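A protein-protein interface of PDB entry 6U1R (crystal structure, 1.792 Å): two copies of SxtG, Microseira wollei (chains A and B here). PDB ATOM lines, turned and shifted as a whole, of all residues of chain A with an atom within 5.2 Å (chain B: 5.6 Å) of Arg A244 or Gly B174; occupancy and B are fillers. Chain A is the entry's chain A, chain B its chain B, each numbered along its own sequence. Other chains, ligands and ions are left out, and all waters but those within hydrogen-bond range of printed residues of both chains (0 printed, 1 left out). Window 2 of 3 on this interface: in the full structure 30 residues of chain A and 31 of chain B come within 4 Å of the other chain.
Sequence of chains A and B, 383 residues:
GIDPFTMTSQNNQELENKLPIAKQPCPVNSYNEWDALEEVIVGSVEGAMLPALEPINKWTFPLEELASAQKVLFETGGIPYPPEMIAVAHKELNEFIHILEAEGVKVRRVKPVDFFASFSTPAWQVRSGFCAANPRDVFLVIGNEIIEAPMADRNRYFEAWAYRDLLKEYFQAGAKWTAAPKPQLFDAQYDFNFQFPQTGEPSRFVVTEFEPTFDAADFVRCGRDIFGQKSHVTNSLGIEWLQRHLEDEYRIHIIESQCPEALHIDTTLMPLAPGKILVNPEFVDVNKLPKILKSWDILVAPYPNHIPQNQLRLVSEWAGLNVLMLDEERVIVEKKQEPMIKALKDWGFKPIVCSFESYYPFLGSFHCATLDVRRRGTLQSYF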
ATOM      1  N   ILE A 239      -1.289  29.350 -15.862  1.00  0.00           N
ATOM      2  CA  ILE A 239      -1.185  29.749 -14.459  1.00  0.00           C
ATOM      3  C   ILE A 239      -2.554  29.710 -13.804  1.00  0.00           C
ATOM      4  O   ILE A 239      -2.706  29.225 -12.671  1.00  0.00           O
ATOM      5  CB  ILE A 239      -0.556  31.153 -14.358  1.00  0.00           C
ATOM      6  CG1 ILE A 239       0.900  31.131 -14.790  1.00  0.00           C
ATOM      7  CG2 ILE A 239      -0.677  31.723 -12.954  1.00  0.00           C
ATOM      8  CD1 ILE A 239       1.470  32.490 -15.059  1.00  0.00           C
ATOM      9  N   GLU A 240      -3.571  30.239 -14.509  1.00  0.00           N
ATOM     10  CA  GLU A 240      -4.943  30.237 -13.998  1.00  0.00           C
ATOM     11  C   GLU A 240      -5.437  28.817 -13.762  1.00  0.00           C
ATOM     12  O   GLU A 240      -6.131  28.536 -12.766  1.00  0.00           O
ATOM     13  CB  GLU A 240      -5.880  30.967 -14.977  1.00  0.00           C
ATOM     14  CG  GLU A 240      -7.298  31.200 -14.430  1.00  0.00           C
ATOM     15  CD  GLU A 240      -8.303  31.752 -15.448  1.00  0.00           C
ATOM     16  OE1 GLU A 240      -7.996  31.844 -16.662  1.00  0.00           O
ATOM     17  OE2 GLU A 240      -9.428  32.089 -15.019  1.00  0.00           O
ATOM     18  N   TRP A 241      -5.076  27.895 -14.663  1.00  0.00           N
ATOM     19  CA  TRP A 241      -5.454  26.501 -14.489  1.00  0.00           C
ATOM     20  C   TRP A 241      -4.840  25.937 -13.214  1.00  0.00           C
ATOM     21  O   TRP A 241      -5.523  25.270 -12.419  1.00  0.00           O
ATOM     22  CB  TRP A 241      -5.041  25.645 -15.703  1.00  0.00           C
ATOM     23  CG  TRP A 241      -5.571  24.260 -15.542  1.00  0.00           C
ATOM     24  CD1 TRP A 241      -6.766  23.779 -16.019  1.00  0.00           C
ATOM     25  CD2 TRP A 241      -4.969  23.179 -14.800  1.00  0.00           C
ATOM     26  NE1 TRP A 241      -6.945  22.471 -15.610  1.00  0.00           N
ATOM     27  CE2 TRP A 241      -5.858  22.082 -14.864  1.00  0.00           C
ATOM     28  CE3 TRP A 241      -3.764  23.038 -14.090  1.00  0.00           C
ATOM     29  CZ2 TRP A 241      -5.575  20.855 -14.245  1.00  0.00           C
ATOM     30  CZ3 TRP A 241      -3.492  21.824 -13.471  1.00  0.00           C
ATOM     31  CH2 TRP A 241      -4.396  20.748 -13.555  1.00  0.00           C
ATOM     32  N   LEU A 242      -3.550  26.194 -12.990  1.00  0.00           N
ATOM     33  CA  LEU A 242      -2.910  25.630 -11.801  1.00  0.00           C
ATOM     34  C   LEU A 242      -3.461  26.262 -10.533  1.00  0.00           C
ATOM     35  O   LEU A 242      -3.647  25.574  -9.522  1.00  0.00           O
ATOM     36  CB  LEU A 242      -1.401  25.805 -11.868  1.00  0.00           C
ATOM     37  CG  LEU A 242      -0.591  25.157 -10.735  1.00  0.00           C
ATOM     38  CD1 LEU A 242      -0.777  23.643 -10.753  1.00  0.00           C
ATOM     39  CD2 LEU A 242       0.873  25.543 -10.873  1.00  0.00           C
ATOM     40  N   GLN A 243      -3.733  27.571 -10.556  1.00  0.00           N
ATOM     41  CA  GLN A 243      -4.309  28.191  -9.365  1.00  0.00           C
ATOM     42  C   GLN A 243      -5.679  27.604  -9.056  1.00  0.00           C
ATOM     43  O   GLN A 243      -5.991  27.351  -7.886  1.00  0.00           O
ATOM     44  CB  GLN A 243      -4.393  29.713  -9.516  1.00  0.00           C
ATOM     45  CG  GLN A 243      -5.020  30.445  -8.289  1.00  0.00           C
ATOM     46  CD  GLN A 243      -4.232  30.273  -6.978  1.00  0.00           C
ATOM     47  OE1 GLN A 243      -3.430  31.149  -6.600  1.00  0.00           O
ATOM     48  NE2 GLN A 243      -4.488  29.162  -6.260  1.00  0.00           N
ATOM     49  N   ARG A 244      -6.495  27.338 -10.076  1.00  0.00           N
ATOM     50  CA  ARG A 244      -7.802  26.754  -9.788  1.00  0.00           C
ATOM     51  C   ARG A 244      -7.665  25.330  -9.272  1.00  0.00           C
ATOM     52  O   ARG A 244      -8.369  24.929  -8.338  1.00  0.00           O
ATOM     53  CB  ARG A 244      -8.703  26.762 -11.011  1.00  0.00           C
ATOM     54  CG  ARG A 244     -10.056  26.082 -10.667  1.00  0.00           C
ATOM     55  CD  ARG A 244     -11.191  26.519 -11.524  1.00  0.00           C
ATOM     56  NE  ARG A 244     -11.271  27.974 -11.633  1.00  0.00           N
ATOM     57  CZ  ARG A 244     -11.694  28.612 -12.716  1.00  0.00           C
ATOM     58  NH1 ARG A 244     -12.088  27.929 -13.787  1.00  0.00           N
ATOM     59  NH2 ARG A 244     -11.716  29.944 -12.730  1.00  0.00           N
ATOM     60  N   HIS A 245      -6.778  24.541  -9.881  1.00  0.00           N
ATOM     61  CA  HIS A 245      -6.585  23.168  -9.431  1.00  0.00           C
ATOM     62  C   HIS A 245      -6.152  23.109  -7.971  1.00  0.00           C
ATOM     63  O   HIS A 245      -6.563  22.193  -7.233  1.00  0.00           O
ATOM     64  CB  HIS A 245      -5.559  22.475 -10.328  1.00  0.00           C
ATOM     65  CG  HIS A 245      -5.427  21.013 -10.059  1.00  0.00           C
ATOM     66  ND1 HIS A 245      -6.410  20.103 -10.395  1.00  0.00           N
ATOM     67  CD2 HIS A 245      -4.437  20.302  -9.471  1.00  0.00           C
ATOM     68  CE1 HIS A 245      -6.020  18.891 -10.033  1.00  0.00           C
ATOM     69  NE2 HIS A 245      -4.825  18.984  -9.477  1.00  0.00           N
ATOM     70  N   LEU A 246      -5.346  24.077  -7.527  1.00  0.00           N
ATOM     71  CA  LEU A 246      -4.772  24.090  -6.184  1.00  0.00           C
ATOM     72  C   LEU A 246      -5.450  25.088  -5.239  1.00  0.00           C
ATOM     73  O   LEU A 246      -4.903  25.379  -4.172  1.00  0.00           O
ATOM     74  CB  LEU A 246      -3.274  24.401  -6.264  1.00  0.00           C
ATOM     75  CG  LEU A 246      -2.401  23.424  -7.053  1.00  0.00           C
ATOM     76  CD1 LEU A 246      -0.936  23.857  -7.004  1.00  0.00           C
ATOM     77  CD2 LEU A 246      -2.607  21.999  -6.552  1.00  0.00           C
ATOM     78  N   GLU A 247      -6.637  25.599  -5.585  1.00  0.00           N
ATOM     79  CA  GLU A 247      -7.174  26.773  -4.883  1.00  0.00           C
ATOM     80  C   GLU A 247      -7.585  26.487  -3.439  1.00  0.00           C
ATOM     81  O   GLU A 247      -7.667  27.426  -2.641  1.00  0.00           O
ATOM     82  CB  GLU A 247      -8.393  27.342  -5.624  1.00  0.00           C
ATOM     83  CG  GLU A 247      -9.601  26.403  -5.640  1.00  0.00           C
ATOM     84  CD  GLU A 247     -10.764  26.924  -6.480  1.00  0.00           C
ATOM     85  OE1 GLU A 247     -10.643  28.017  -7.078  1.00  0.00           O
ATOM     86  OE2 GLU A 247     -11.787  26.217  -6.560  1.00  0.00           O
ATOM     87  N   CYS B  26     -21.840  28.782 -11.229  1.00  0.00           N
ATOM     88  CA  CYS B  26     -20.948  28.419 -12.329  1.00  0.00           C
ATOM     89  C   CYS B  26     -21.746  27.665 -13.420  1.00  0.00           C
ATOM     90  O   CYS B  26     -22.699  26.955 -13.111  1.00  0.00           O
ATOM     91  CB  CYS B  26     -19.773  27.609 -11.753  1.00  0.00           C
ATOM     92  SG  CYS B  26     -18.887  26.448 -12.814  1.00  0.00           S
ATOM     93  N   PRO B  27     -21.396  27.851 -14.698  1.00  0.00           N
ATOM     94  CA  PRO B  27     -22.213  27.252 -15.770  1.00  0.00           C
ATOM     95  C   PRO B  27     -22.195  25.735 -15.791  1.00  0.00           C
ATOM     96  O   PRO B  27     -23.101  25.146 -16.396  1.00  0.00           O
ATOM     97  CB  PRO B  27     -21.581  27.809 -17.045  1.00  0.00           C
ATOM     98  CG  PRO B  27     -20.152  28.019 -16.653  1.00  0.00           C
ATOM     99  CD  PRO B  27     -20.255  28.590 -15.257  1.00  0.00           C
ATOM    100  N   ASN B 144     -19.148  20.746 -10.487  1.00  0.00           N
ATOM    101  CA  ASN B 144     -18.630  21.811 -11.332  1.00  0.00           C
ATOM    102  C   ASN B 144     -17.357  21.410 -12.075  1.00  0.00           C
ATOM    103  O   ASN B 144     -16.691  22.283 -12.650  1.00  0.00           O
ATOM    104  CB  ASN B 144     -18.370  23.068 -10.495  1.00  0.00           C
ATOM    105  CG  ASN B 144     -17.183  22.918  -9.598  1.00  0.00           C
ATOM    106  OD1 ASN B 144     -16.849  21.811  -9.175  1.00  0.00           O
ATOM    107  ND2 ASN B 144     -16.523  24.035  -9.296  1.00  0.00           N
ATOM    108  N   GLU B 169     -14.424  27.728 -22.734  1.00  0.00           N
ATOM    109  CA  GLU B 169     -15.458  28.674 -22.313  1.00  0.00           C
ATOM    110  C   GLU B 169     -15.914  28.392 -20.886  1.00  0.00           C
ATOM    111  O   GLU B 169     -16.014  29.303 -20.052  1.00  0.00           O
ATOM    112  CB  GLU B 169     -16.640  28.611 -23.287  1.00  0.00           C
ATOM    113  CG  GLU B 169     -17.884  29.402 -22.823  1.00  0.00           C
ATOM    114  CD  GLU B 169     -19.141  29.115 -23.637  1.00  0.00           C
ATOM    115  OE1 GLU B 169     -19.045  29.025 -24.882  1.00  0.00           O
ATOM    116  OE2 GLU B 169     -20.229  28.978 -23.016  1.00  0.00           O
ATOM    117  N   TYR B 170     -16.186  27.121 -20.574  1.00  0.00           N
ATOM    118  CA  TYR B 170     -16.668  26.794 -19.234  1.00  0.00           C
ATOM    119  C   TYR B 170     -15.599  27.073 -18.182  1.00  0.00           C
ATOM    120  O   TYR B 170     -15.904  27.566 -17.089  1.00  0.00           O
ATOM    121  CB  TYR B 170     -17.102  25.330 -19.180  1.00  0.00           C
ATOM    122  CG  TYR B 170     -18.321  24.984 -20.027  1.00  0.00           C
ATOM    123  CD1 TYR B 170     -19.458  25.816 -20.063  1.00  0.00           C
ATOM    124  CD2 TYR B 170     -18.353  23.815 -20.773  1.00  0.00           C
ATOM    125  CE1 TYR B 170     -20.567  25.478 -20.828  1.00  0.00           C
ATOM    126  CE2 TYR B 170     -19.449  23.485 -21.541  1.00  0.00           C
ATOM    127  CZ  TYR B 170     -20.556  24.308 -21.554  1.00  0.00           C
ATOM    128  OH  TYR B 170     -21.653  23.952 -22.319  1.00  0.00           O
ATOM    129  N   PHE B 171     -14.338  26.756 -18.501  1.00  0.00           N
ATOM    130  CA  PHE B 171     -13.234  27.063 -17.595  1.00  0.00           C
ATOM    131  C   PHE B 171     -13.132  28.569 -17.343  1.00  0.00           C
ATOM    132  O   PHE B 171     -12.948  29.014 -16.202  1.00  0.00           O
ATOM    133  CB  PHE B 171     -11.929  26.517 -18.181  1.00  0.00           C
ATOM    134  CG  PHE B 171     -10.715  26.895 -17.374  1.00  0.00           C
ATOM    135  CD1 PHE B 171     -10.414  26.219 -16.211  1.00  0.00           C
ATOM    136  CD2 PHE B 171      -9.894  27.945 -17.779  1.00  0.00           C
ATOM    137  CE1 PHE B 171      -9.329  26.573 -15.440  1.00  0.00           C
ATOM    138  CE2 PHE B 171      -8.794  28.292 -17.023  1.00  0.00           C
ATOM    139  CZ  PHE B 171      -8.515  27.605 -15.846  1.00  0.00           C
ATOM    140  N   GLN B 172     -13.245  29.363 -18.407  1.00  0.00           N
ATOM    141  CA  GLN B 172     -13.234  30.817 -18.295  1.00  0.00           C
ATOM    142  C   GLN B 172     -14.357  31.332 -17.411  1.00  0.00           C
ATOM    143  O   GLN B 172     -14.233  32.414 -16.821  1.00  0.00           O
ATOM    144  CB  GLN B 172     -13.332  31.406 -19.701  1.00  0.00           C
ATOM    145  CG  GLN B 172     -13.442  32.910 -19.795  1.00  0.00           C
ATOM    146  CD  GLN B 172     -13.541  33.341 -21.237  1.00  0.00           C
ATOM    147  OE1 GLN B 172     -14.573  33.134 -21.887  1.00  0.00           O
ATOM    148  NE2 GLN B 172     -12.458  33.896 -21.768  1.00  0.00           N
ATOM    149  N   ALA B 173     -15.456  30.587 -17.307  1.00  0.00           N
ATOM    150  CA  ALA B 173     -16.591  30.969 -16.489  1.00  0.00           C
ATOM    151  C   ALA B 173     -16.580  30.318 -15.108  1.00  0.00           C
ATOM    152  O   ALA B 173     -17.559  30.460 -14.371  1.00  0.00           O
ATOM    153  CB  ALA B 173     -17.891  30.632 -17.219  1.00  0.00           C
ATOM    154  N   GLY B 174     -15.511  29.606 -14.740  1.00  0.00           N
ATOM    155  CA  GLY B 174     -15.339  29.132 -13.369  1.00  0.00           C
ATOM    156  C   GLY B 174     -15.296  27.624 -13.181  1.00  0.00           C
ATOM    157  O   GLY B 174     -15.103  27.162 -12.042  1.00  0.00           O
ATOM    158  N   ALA B 175     -15.463  26.833 -14.231  1.00  0.00           N
ATOM    159  CA  ALA B 175     -15.538  25.389 -14.083  1.00  0.00           C
ATOM    160  C   ALA B 175     -14.168  24.806 -13.783  1.00  0.00           C
ATOM    161  O   ALA B 175     -13.136  25.336 -14.207  1.00  0.00           O
ATOM    162  CB  ALA B 175     -16.094  24.768 -15.356  1.00  0.00           C
ATOM    163  N   LYS B 176     -14.162  23.700 -13.042  1.00  0.00           N
ATOM    164  CA  LYS B 176     -12.955  22.909 -12.889  1.00  0.00           C
ATOM    165  C   LYS B 176     -12.851  21.965 -14.070  1.00  0.00           C
ATOM    166  O   LYS B 176     -13.862  21.499 -14.601  1.00  0.00           O
ATOM    167  CB  LYS B 176     -12.969  22.104 -11.588  1.00  0.00           C
ATOM    168  CG  LYS B 176     -12.866  22.933 -10.340  1.00  0.00           C
ATOM    169  CD  LYS B 176     -12.948  22.037  -9.095  1.00  0.00           C
ATOM    170  CE  LYS B 176     -13.200  22.841  -7.828  1.00  0.00           C
ATOM    171  NZ  LYS B 176     -13.419  21.961  -6.621  1.00  0.00           N
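No position is printed for both chains.
Of the 6 pairs that touch across the chains among the printed residues, none has its exchanged pair printed and touching as well.
Arg A244 touches just these residues of chain B: Phe B171, Gly B174 and Ala B175.
Of chain A, only Arg A244 (3.3 Å) comes within 4 Å of Gly B174.
Of the printed residues of chain A, Ala B175 touches Arg A244.
Of the printed residues of chain A, Phe B171 touches Glu A240, Trp A241 and Arg A244.
Of the printed residues of chain B, Trp A241 touches Phe B171 (3.5 Å).
Printed residues of chain B within 4 Å of Glu A247: Lys B176 (3.9 Å).
Of the printed residues of chain B, Glu A240 touches Phe B171 (3.7 Å).
The nearest residue of chain B that does not touch Arg A244 is Lys B176 (4.1 Å).
The nearest printed residue of chain A that does not touch Gly B174 is Glu A247 (6.5 Å).
The guanidinium group (NH1) of Arg A244 is in hydrogen-bond range of the backbone carbonyl oxygen (O) of Ala B175 (2.8 Å).
The backbone carbonyl oxygen (O) of Phe B171 sits at hydrogen-bond distance from the guanidinium group (NH1) of Arg A244.
The side-chain carboxylate (OE2) of Glu A240 lies within salt-bridge range of the guanidinium group (NH2) of Arg A244 (3.9 Å).
O of Asn B144 is in hydrogen-bond range of N of Lys B176 (2.9 Å).
The backbone carbonyl oxygen (O) of Tyr B170 sits at hydrogen-bond distance from the backbone NH (N) of Ala B175, at 3.0 Å.
The side-chain sulfur (SG) of Cys B26 sits at hydrogen-bond distance from the backbone NH (N) of Ala B175, at 3.7 Å.
Among the printed residues, merely in contact across the chains: Arg A244 with Gly B174 (3.3 Å), Trp A241 with Phe B171 (3.5 Å), Glu A240 with Phe B171 (3.7 Å) and Glu A247 with Lys B176 (3.9 Å).
Hydrophobic or aromatic side chains of chain A within 4 Å of the printed part of chain B: Trp A241.
Of the 11 printed residues of chain B, 4 touch a printed residue of chain A.
Hydrophobic or aromatic side chains of chain B within 4 Å of the printed part of chain A: Phe B171.
Along chain B the printed residues that touch a printed residue of chain A span positions 171 to 176.
Among the printed residues, no Asp or Glu carboxylate lies within 4 Å of a Lys or Arg side-chain nitrogen of the other chain.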
